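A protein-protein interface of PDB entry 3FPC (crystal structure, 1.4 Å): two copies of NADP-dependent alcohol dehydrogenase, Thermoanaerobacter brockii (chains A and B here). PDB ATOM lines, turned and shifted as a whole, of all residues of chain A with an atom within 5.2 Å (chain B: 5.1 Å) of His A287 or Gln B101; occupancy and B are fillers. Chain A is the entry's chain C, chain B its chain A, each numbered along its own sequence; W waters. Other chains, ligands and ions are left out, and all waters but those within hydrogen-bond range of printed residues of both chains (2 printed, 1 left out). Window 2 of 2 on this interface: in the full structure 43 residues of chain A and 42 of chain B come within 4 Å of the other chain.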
ATOM      1  N   PRO A 258      -3.355  10.243 -21.079  1.00  0.00           N
ATOM      2  CA  PRO A 258      -3.446   9.677 -22.420  1.00  0.00           C
ATOM      3  C   PRO A 258      -2.607   8.403 -22.468  1.00  0.00           C
ATOM      4  O   PRO A 258      -1.581   8.289 -21.769  1.00  0.00           O
ATOM      5  CB  PRO A 258      -2.885  10.783 -23.316  1.00  0.00           C
ATOM      6  CG  PRO A 258      -1.959  11.554 -22.431  1.00  0.00           C
ATOM      7  CD  PRO A 258      -2.582  11.480 -21.059  1.00  0.00           C
ATOM      8  N   GLY A 259      -3.008   7.439 -23.285  1.00  0.00           N
ATOM      9  CA  GLY A 259      -2.285   6.174 -23.309  1.00  0.00           C
ATOM     10  C   GLY A 259      -2.542   5.393 -22.059  1.00  0.00           C
ATOM     11  O   GLY A 259      -1.694   5.330 -21.168  1.00  0.00           O
ATOM     12  N   SER A 260      -3.738   4.847 -21.948  1.00  0.00           N
ATOM     13  CA  SER A 260      -4.201   4.323 -20.686  1.00  0.00           C
ATOM     14  C   SER A 260      -5.362   3.395 -20.919  1.00  0.00           C
ATOM     15  O   SER A 260      -5.814   3.205 -22.058  1.00  0.00           O
ATOM     16  CB  SER A 260      -4.640   5.476 -19.796  1.00  0.00           C
ATOM     17  OG  SER A 260      -5.688   6.170 -20.427  1.00  0.00           O
ATOM     18  N   MET A 285      -8.483  10.480 -30.271  1.00  0.00           N
ATOM     19  CA  MET A 285      -7.132  10.080 -30.603  1.00  0.00           C
ATOM     20  C   MET A 285      -6.207  10.015 -29.381  1.00  0.00           C
ATOM     21  O   MET A 285      -4.995   9.940 -29.528  1.00  0.00           O
ATOM     22  CB  MET A 285      -6.549  11.017 -31.684  1.00  0.00           C
ATOM     23  CG  MET A 285      -7.358  11.037 -32.965  1.00  0.00           C
ATOM     24  SD  MET A 285      -6.620  12.067 -34.230  1.00  0.00           S
ATOM     25  CE  MET A 285      -6.909  13.690 -33.502  1.00  0.00           C
ATOM     26  N   GLY A 286      -6.776  10.015 -28.174  1.00  0.00           N
ATOM     27  CA  GLY A 286      -5.988  10.058 -26.962  1.00  0.00           C
ATOM     28  C   GLY A 286      -5.453   8.753 -26.399  1.00  0.00           C
ATOM     29  O   GLY A 286      -4.827   8.757 -25.333  1.00  0.00           O
ATOM     30  N   HIS A 287      -5.704   7.650 -27.091  1.00  0.00           N
ATOM     31  CA  HIS A 287      -5.382   6.307 -26.598  1.00  0.00           C
ATOM     32  C   HIS A 287      -5.858   6.022 -25.175  1.00  0.00           C
ATOM     33  O   HIS A 287      -5.160   5.373 -24.388  1.00  0.00           O
ATOM     34  CB  HIS A 287      -3.895   6.006 -26.745  1.00  0.00           C
ATOM     35  CG  HIS A 287      -3.394   5.908 -28.160  1.00  0.00           C
ATOM     36  ND1 HIS A 287      -2.819   6.965 -28.830  1.00  0.00           N
ATOM     37  CD2 HIS A 287      -3.333   4.844 -29.009  1.00  0.00           C
ATOM     38  CE1 HIS A 287      -2.431   6.547 -30.027  1.00  0.00           C
ATOM     39  NE2 HIS A 287      -2.730   5.266 -30.161  1.00  0.00           N
ATOM     40  N   LYS A 288      -7.047   6.523 -24.855  1.00  0.00           N
ATOM     41  CA  LYS A 288      -7.696   6.202 -23.590  1.00  0.00           C
ATOM     42  C   LYS A 288      -8.644   5.056 -23.839  1.00  0.00           C
ATOM     43  O   LYS A 288      -9.782   5.243 -24.255  1.00  0.00           O
ATOM     44  CB  LYS A 288      -8.385   7.447 -22.994  1.00  0.00           C
ATOM     45  CG  LYS A 288      -7.410   8.592 -22.660  1.00  0.00           C
ATOM     46  CD  LYS A 288      -8.108   9.778 -22.040  1.00  0.00           C
ATOM     47  CE  LYS A 288      -7.125  10.826 -21.588  1.00  0.00           C
ATOM     48  NZ  LYS A 288      -7.803  11.996 -20.921  1.00  0.00           N
ATOM     49  N   HIS A 289      -8.110   3.848 -23.722  1.00  0.00           N
ATOM     50  CA  HIS A 289      -8.830   2.616 -24.084  1.00  0.00           C
ATOM     51  C   HIS A 289      -9.929   2.323 -23.089  1.00  0.00           C
ATOM     52  O   HIS A 289      -9.698   2.479 -21.894  1.00  0.00           O
ATOM     53  CB  HIS A 289      -7.861   1.446 -24.169  1.00  0.00           C
ATOM     54  CG  HIS A 289      -6.693   1.674 -25.061  1.00  0.00           C
ATOM     55  ND1 HIS A 289      -6.799   1.670 -26.421  1.00  0.00           N
ATOM     56  CD2 HIS A 289      -5.386   1.850 -24.792  1.00  0.00           C
ATOM     57  CE1 HIS A 289      -5.609   1.900 -26.961  1.00  0.00           C
ATOM     58  NE2 HIS A 289      -4.732   2.006 -25.986  1.00  0.00           N
ATOM     59  N   ILE B  86       3.706  13.082 -37.257  1.00  0.00           N
ATOM     60  CA  ILE B  86       4.011  13.030 -35.822  1.00  0.00           C
ATOM     61  C   ILE B  86       5.536  12.989 -35.674  1.00  0.00           C
ATOM     62  O   ILE B  86       6.210  12.069 -36.187  1.00  0.00           O
ATOM     63  CB  ILE B  86       3.284  11.828 -35.191  1.00  0.00           C
ATOM     64  CG1 ILE B  86       1.801  12.160 -34.873  1.00  0.00           C
ATOM     65  CG2 ILE B  86       3.952  11.335 -33.874  1.00  0.00           C
ATOM     66  CD1 ILE B  86       0.933  12.785 -36.019  1.00  0.00           C
ATOM     67  N   GLY B  98       5.631   4.054 -23.552  1.00  0.00           N
ATOM     68  CA  GLY B  98       5.186   3.467 -24.824  1.00  0.00           C
ATOM     69  C   GLY B  98       4.216   4.245 -25.687  1.00  0.00           C
ATOM     70  O   GLY B  98       3.606   3.675 -26.578  1.00  0.00           O
ATOM     71  N   TYR B  99       4.099   5.542 -25.455  1.00  0.00           N
ATOM     72  CA  TYR B  99       3.147   6.385 -26.191  1.00  0.00           C
ATOM     73  C   TYR B  99       3.784   7.657 -26.701  1.00  0.00           C
ATOM     74  O   TYR B  99       3.490   8.769 -26.238  1.00  0.00           O
ATOM     75  CB  TYR B  99       1.940   6.702 -25.321  1.00  0.00           C
ATOM     76  CG  TYR B  99       0.958   5.577 -25.162  1.00  0.00           C
ATOM     77  CD1 TYR B  99       0.086   5.237 -26.184  1.00  0.00           C
ATOM     78  CD2 TYR B  99       0.940   4.800 -24.008  1.00  0.00           C
ATOM     79  CE1 TYR B  99      -0.843   4.194 -26.020  1.00  0.00           C
ATOM     80  CE2 TYR B  99       0.048   3.733 -23.875  1.00  0.00           C
ATOM     81  CZ  TYR B  99      -0.844   3.446 -24.872  1.00  0.00           C
ATOM     82  OH  TYR B  99      -1.763   2.377 -24.735  1.00  0.00           O
ATOM     83  N   HIS B 100       4.641   7.513 -27.693  1.00  0.00           N
ATOM     84  CA  HIS B 100       5.323   8.697 -28.252  1.00  0.00           C
ATOM     85  C   HIS B 100       4.364   9.728 -28.845  1.00  0.00           C
ATOM     86  O   HIS B 100       4.684  10.908 -28.912  1.00  0.00           O
ATOM     87  CB  HIS B 100       6.365   8.314 -29.293  1.00  0.00           C
ATOM     88  CG  HIS B 100       5.804   7.834 -30.601  1.00  0.00           C
ATOM     89  ND1 HIS B 100       5.915   6.534 -31.005  1.00  0.00           N
ATOM     90  CD2 HIS B 100       5.198   8.500 -31.623  1.00  0.00           C
ATOM     91  CE1 HIS B 100       5.386   6.404 -32.216  1.00  0.00           C
ATOM     92  NE2 HIS B 100       4.940   7.581 -32.608  1.00  0.00           N
ATOM     93  N   GLN B 101       3.166   9.294 -29.242  1.00  0.00           N
ATOM     94  CA  GLN B 101       2.151  10.201 -29.788  1.00  0.00           C
ATOM     95  C   GLN B 101       1.745  11.289 -28.820  1.00  0.00           C
ATOM     96  O   GLN B 101       1.306  12.349 -29.238  1.00  0.00           O
ATOM     97  CB  GLN B 101       0.862   9.444 -30.182  1.00  0.00           C
ATOM     98  CG  GLN B 101       1.057   8.513 -31.315  1.00  0.00           C
ATOM     99  CD  GLN B 101       1.239   7.100 -30.884  1.00  0.00           C
ATOM    100  OE1 GLN B 101       1.963   6.805 -29.897  1.00  0.00           O
ATOM    101  NE2 GLN B 101       0.600   6.182 -31.624  1.00  0.00           N
ATOM    102  N   HIS B 102       1.910  10.999 -27.537  1.00  0.00           N
ATOM    103  CA  HIS B 102       1.472  11.874 -26.461  1.00  0.00           C
ATOM    104  C   HIS B 102       2.657  12.396 -25.677  1.00  0.00           C
ATOM    105  O   HIS B 102       2.540  12.791 -24.512  1.00  0.00           O
ATOM    106  CB  HIS B 102       0.460  11.147 -25.570  1.00  0.00           C
ATOM    107  CG  HIS B 102      -0.663  10.583 -26.366  1.00  0.00           C
ATOM    108  ND1 HIS B 102      -1.497  11.386 -27.127  1.00  0.00           N
ATOM    109  CD2 HIS B 102      -1.016   9.294 -26.630  1.00  0.00           C
ATOM    110  CE1 HIS B 102      -2.317  10.600 -27.826  1.00  0.00           C
ATOM    111  NE2 HIS B 102      -2.043   9.327 -27.542  1.00  0.00           N
ATOM    112  N   SER B 103       3.802  12.456 -26.358  1.00  0.00           N
ATOM    113  CA  SER B 103       5.005  12.968 -25.730  1.00  0.00           C
ATOM    114  C   SER B 103       4.888  14.462 -25.403  1.00  0.00           C
ATOM    115  O   SER B 103       4.779  15.301 -26.274  1.00  0.00           O
ATOM    116  CB  SER B 103       6.211  12.728 -26.613  1.00  0.00           C
ATOM    117  OG  SER B 103       7.353  13.183 -25.941  1.00  0.00           O
ATOM    118  N   GLY B 105       2.322  15.559 -23.565  1.00  0.00           N
ATOM    119  CA  GLY B 105       0.914  15.827 -23.389  1.00  0.00           C
ATOM    120  C   GLY B 105       0.048  15.188 -24.457  1.00  0.00           C
ATOM    121  O   GLY B 105       0.550  14.749 -25.501  1.00  0.00           O
ATOM    122  N   LEU B 107      -1.811  14.313 -27.503  1.00  0.00           N
ATOM    123  CA  LEU B 107      -1.663  14.692 -28.919  1.00  0.00           C
ATOM    124  C   LEU B 107      -0.385  15.454 -29.234  1.00  0.00           C
ATOM    125  O   LEU B 107      -0.167  15.831 -30.389  1.00  0.00           O
ATOM    126  CB  LEU B 107      -2.855  15.494 -29.495  1.00  0.00           C
ATOM    127  CG  LEU B 107      -4.236  14.954 -29.245  1.00  0.00           C
ATOM    128  CD1 LEU B 107      -5.282  15.831 -30.011  1.00  0.00           C
ATOM    129  CD2 LEU B 107      -4.370  13.480 -29.647  1.00  0.00           C
ATOM    130  N   ALA B 108       0.492  15.657 -28.258  1.00  0.00           N
ATOM    131  CA  ALA B 108       1.601  16.597 -28.426  1.00  0.00           C
ATOM    132  C   ALA B 108       2.744  16.074 -29.320  1.00  0.00           C
ATOM    133  O   ALA B 108       3.649  16.831 -29.715  1.00  0.00           O
ATOM    134  CB  ALA B 108       2.133  17.084 -27.060  1.00  0.00           C
ATOM    135  N   GLY B 109       2.730  14.781 -29.652  1.00  0.00           N
ATOM    136  CA  GLY B 109       3.647  14.273 -30.672  1.00  0.00           C
ATOM    137  C   GLY B 109       3.324  14.782 -32.058  1.00  0.00           C
ATOM    138  O   GLY B 109       4.179  14.792 -32.950  1.00  0.00           O
ATOM    139  N   TRP B 110       2.060  15.167 -32.249  1.00  0.00           N
ATOM    140  CA  TRP B 110       1.593  15.796 -33.474  1.00  0.00           C
ATOM    141  C   TRP B 110       1.826  17.273 -33.324  1.00  0.00           C
ATOM    142  O   TRP B 110       1.076  17.960 -32.654  1.00  0.00           O
ATOM    143  CB  TRP B 110       0.118  15.460 -33.714  1.00  0.00           C
ATOM    144  CG  TRP B 110      -0.531  16.225 -34.830  1.00  0.00           C
ATOM    145  CD1 TRP B 110       0.049  16.683 -35.978  1.00  0.00           C
ATOM    146  CD2 TRP B 110      -1.900  16.616 -34.882  1.00  0.00           C
ATOM    147  NE1 TRP B 110      -0.875  17.355 -36.736  1.00  0.00           N
ATOM    148  CE2 TRP B 110      -2.079  17.340 -36.075  1.00  0.00           C
ATOM    149  CE3 TRP B 110      -2.999  16.440 -34.018  1.00  0.00           C
ATOM    150  CZ2 TRP B 110      -3.320  17.874 -36.438  1.00  0.00           C
ATOM    151  CZ3 TRP B 110      -4.234  16.979 -34.385  1.00  0.00           C
ATOM    152  CH2 TRP B 110      -4.370  17.702 -35.571  1.00  0.00           C
ATOM    153  N   HIS B 157      -2.926   2.359 -38.541  1.00  0.00           N
ATOM    154  CA  HIS B 157      -3.148   2.366 -37.082  1.00  0.00           C
ATOM    155  C   HIS B 157      -4.583   2.025 -36.740  1.00  0.00           C
ATOM    156  O   HIS B 157      -4.841   1.446 -35.705  1.00  0.00           O
ATOM    157  CB  HIS B 157      -2.755   3.717 -36.478  1.00  0.00           C
ATOM    158  CG  HIS B 157      -2.539   3.661 -34.987  1.00  0.00           C
ATOM    159  ND1 HIS B 157      -1.751   2.698 -34.390  1.00  0.00           N
ATOM    160  CD2 HIS B 157      -2.990   4.463 -33.990  1.00  0.00           C
ATOM    161  CE1 HIS B 157      -1.732   2.921 -33.078  1.00  0.00           C
ATOM    162  NE2 HIS B 157      -2.469   3.994 -32.812  1.00  0.00           N
ATOM    163  N   LEU B 161      -5.294  -0.801 -34.069  1.00  0.00           N
ATOM    164  CA  LEU B 161      -6.136  -0.584 -32.895  1.00  0.00           C
ATOM    165  C   LEU B 161      -7.342  -1.514 -32.864  1.00  0.00           C
ATOM    166  O   LEU B 161      -7.833  -1.849 -31.790  1.00  0.00           O
ATOM    167  CB  LEU B 161      -6.605   0.863 -32.825  1.00  0.00           C
ATOM    168  CG  LEU B 161      -5.563   1.917 -32.532  1.00  0.00           C
ATOM    169  CD1 LEU B 161      -6.145   3.310 -32.749  1.00  0.00           C
ATOM    170  CD2 LEU B 161      -4.970   1.757 -31.131  1.00  0.00           C
ATOM    171  N   GLY B 292      -9.220   4.564 -29.505  1.00  0.00           N
ATOM    172  CA  GLY B 292      -9.124   5.704 -30.388  1.00  0.00           C
ATOM    173  C   GLY B 292      -7.790   6.390 -30.213  1.00  0.00           C
ATOM    174  O   GLY B 292      -7.465   6.859 -29.115  1.00  0.00           O
ATOM    175  N   GLY B 293      -7.005   6.421 -31.277  1.00  0.00           N
ATOM    176  CA  GLY B 293      -5.630   6.825 -31.188  1.00  0.00           C
ATOM    177  C   GLY B 293      -5.063   7.611 -32.366  1.00  0.00           C
ATOM    178  O   GLY B 293      -5.324   7.308 -33.525  1.00  0.00           O
ATOM    179  N   LEU B 294      -4.192   8.556 -32.021  1.00  0.00           N
ATOM    180  CA  LEU B 294      -3.364   9.288 -32.956  1.00  0.00           C
ATOM    181  C   LEU B 294      -2.335   8.401 -33.614  1.00  0.00           C
ATOM    182  O   LEU B 294      -1.742   7.548 -32.975  1.00  0.00           O
ATOM    183  CB  LEU B 294      -2.684  10.423 -32.172  1.00  0.00           C
ATOM    184  CG  LEU B 294      -1.742  11.384 -32.916  1.00  0.00           C
ATOM    185  CD1 LEU B 294      -2.515  12.176 -33.936  1.00  0.00           C
ATOM    186  CD2 LEU B 294      -1.090  12.352 -31.906  1.00  0.00           C
ATOM    187  N   CYS B 295      -2.057   8.635 -34.891  1.00  0.00           N
ATOM    188  CA  CYS B 295      -1.128   7.780 -35.619  1.00  0.00           C
ATOM    189  C   CYS B 295       0.302   7.813 -35.068  1.00  0.00           C
ATOM    190  O   CYS B 295       0.779   8.849 -34.607  1.00  0.00           O
ATOM    191  CB  CYS B 295      -1.069   8.149 -37.100  1.00  0.00           C
ATOM    192  SG  CYS B 295      -0.511   9.812 -37.448  1.00  0.00           S
ATOM    193  N   PRO B 296       1.008   6.682 -35.143  1.00  0.00           N
ATOM    194  CA  PRO B 296       2.432   6.710 -34.905  1.00  0.00           C
ATOM    195  C   PRO B 296       3.200   7.569 -35.897  1.00  0.00           C
ATOM    196  O   PRO B 296       2.780   7.732 -37.045  1.00  0.00           O
ATOM    197  CB  PRO B 296       2.857   5.243 -35.027  1.00  0.00           C
ATOM    198  CG  PRO B 296       1.575   4.463 -34.771  1.00  0.00           C
ATOM    199  CD  PRO B 296       0.513   5.312 -35.374  1.00  0.00           C
HETATM  200  O   HOH W   1      -8.085   4.381 -26.960  1.00  0.00           O
HETATM  201  O   HOH W   2      -5.991   9.130 -35.566  1.00  0.00           O
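His A287 touches seven residues of chain B. Printed residues of chain A within 4 Å of Gln B101: His A287 (3.4 Å). Of the printed residues of chain A, His B102 touches Pro A258, Met A285, Gly A286 and His A287. Of the printed residues of chain A, Gly B293 touches Met A285 (3.6 Å) and His A287 (3.4 Å). Of the printed residues of chain A, Leu B294 touches Met A285 (3.0 Å) and His A287 (3.2 Å). The nearest printed residue of chain A that does not touch Gln B101 is Met A285 (5.9 Å). The nearest printed residue of chain A that does not touch Gly B292 is Lys A288 (4.3 Å).
No position is printed for both chains.
The backbone NH (N) of Gly B109 sits at hydrogen-bond distance from the backbone carbonyl oxygen (O) of Gln B101, 2.8 Å away. A ring nitrogen (ND1) of His B102 sits at hydrogen-bond distance from the backbone NH (N) of Leu B107 (3.0 Å). O of Gly A286 lies within hydrogen-bond range of N of Gly A259, 3.0 Å away. O of His A287 lies close to N of Gly A259, 3.2 Å away. O of His A287 sits at hydrogen-bond distance from N of Ser A260, at 2.9 Å. O of Ser A260 is in hydrogen-bond range of N of His A289, 2.9 Å away.
Among the printed residues, pairs that only touch across the chains: Pro A258 with His B102 (3.8 Å), Gly A259 with Tyr B99 (3.4 Å), Met A285 with His B102 (3.2 Å), Met A285 with Leu B107 (3.6 Å), Met A285 with Gly B292 (3.4 Å), Met A285 with Gly B293 (3.6 Å), Gly A286 with His B102 (3.6 Å), His A287 with Tyr B99 (3.6 Å), His A287 with Gln B101 (3.4 Å), His A287 with Gly B293 (3.4 Å) and His A287 with Leu B294 (3.2 Å).
A ring nitrogen (NE2) of His A289 sits at hydrogen-bond distance from the side-chain hydroxyl (OH) of Tyr B99 (3.2 Å). A ring nitrogen (ND1) of His A287 sits at hydrogen-bond distance from a ring nitrogen (NE2) of His B102, at 2.8 Å. A ring nitrogen (NE2) of His B157 sits at hydrogen-bond distance from a ring nitrogen (NE2) of His A287 (3.0 Å). The backbone carbonyl oxygen of Gly B292 sits at hydrogen-bond distance from the backbone NH of Gly A286 (3.4 Å). The backbone carbonyl oxygen (O) of Gly B292 lies within hydrogen-bond range of the backbone NH (N) of His A287, 2.8 Å away. The backbone NH (N) of Leu B294 sits at hydrogen-bond distance from the backbone carbonyl oxygen (O) of Met A285 (3.0 Å).
Among the printed residues, no Asp or Glu carboxylate lies within 4 Å of a Lys or Arg side-chain nitrogen of the other chain.
Water W1 lies within hydrogen-bond range of the backbone NH of Gly B292, a ring nitrogen (ND1) of His A289 and the backbone NH of Lys A288. Water W2 lies within hydrogen-bond range of O of Gly B293 (2.8 Å) and SD of Met A285 (3.3 Å).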
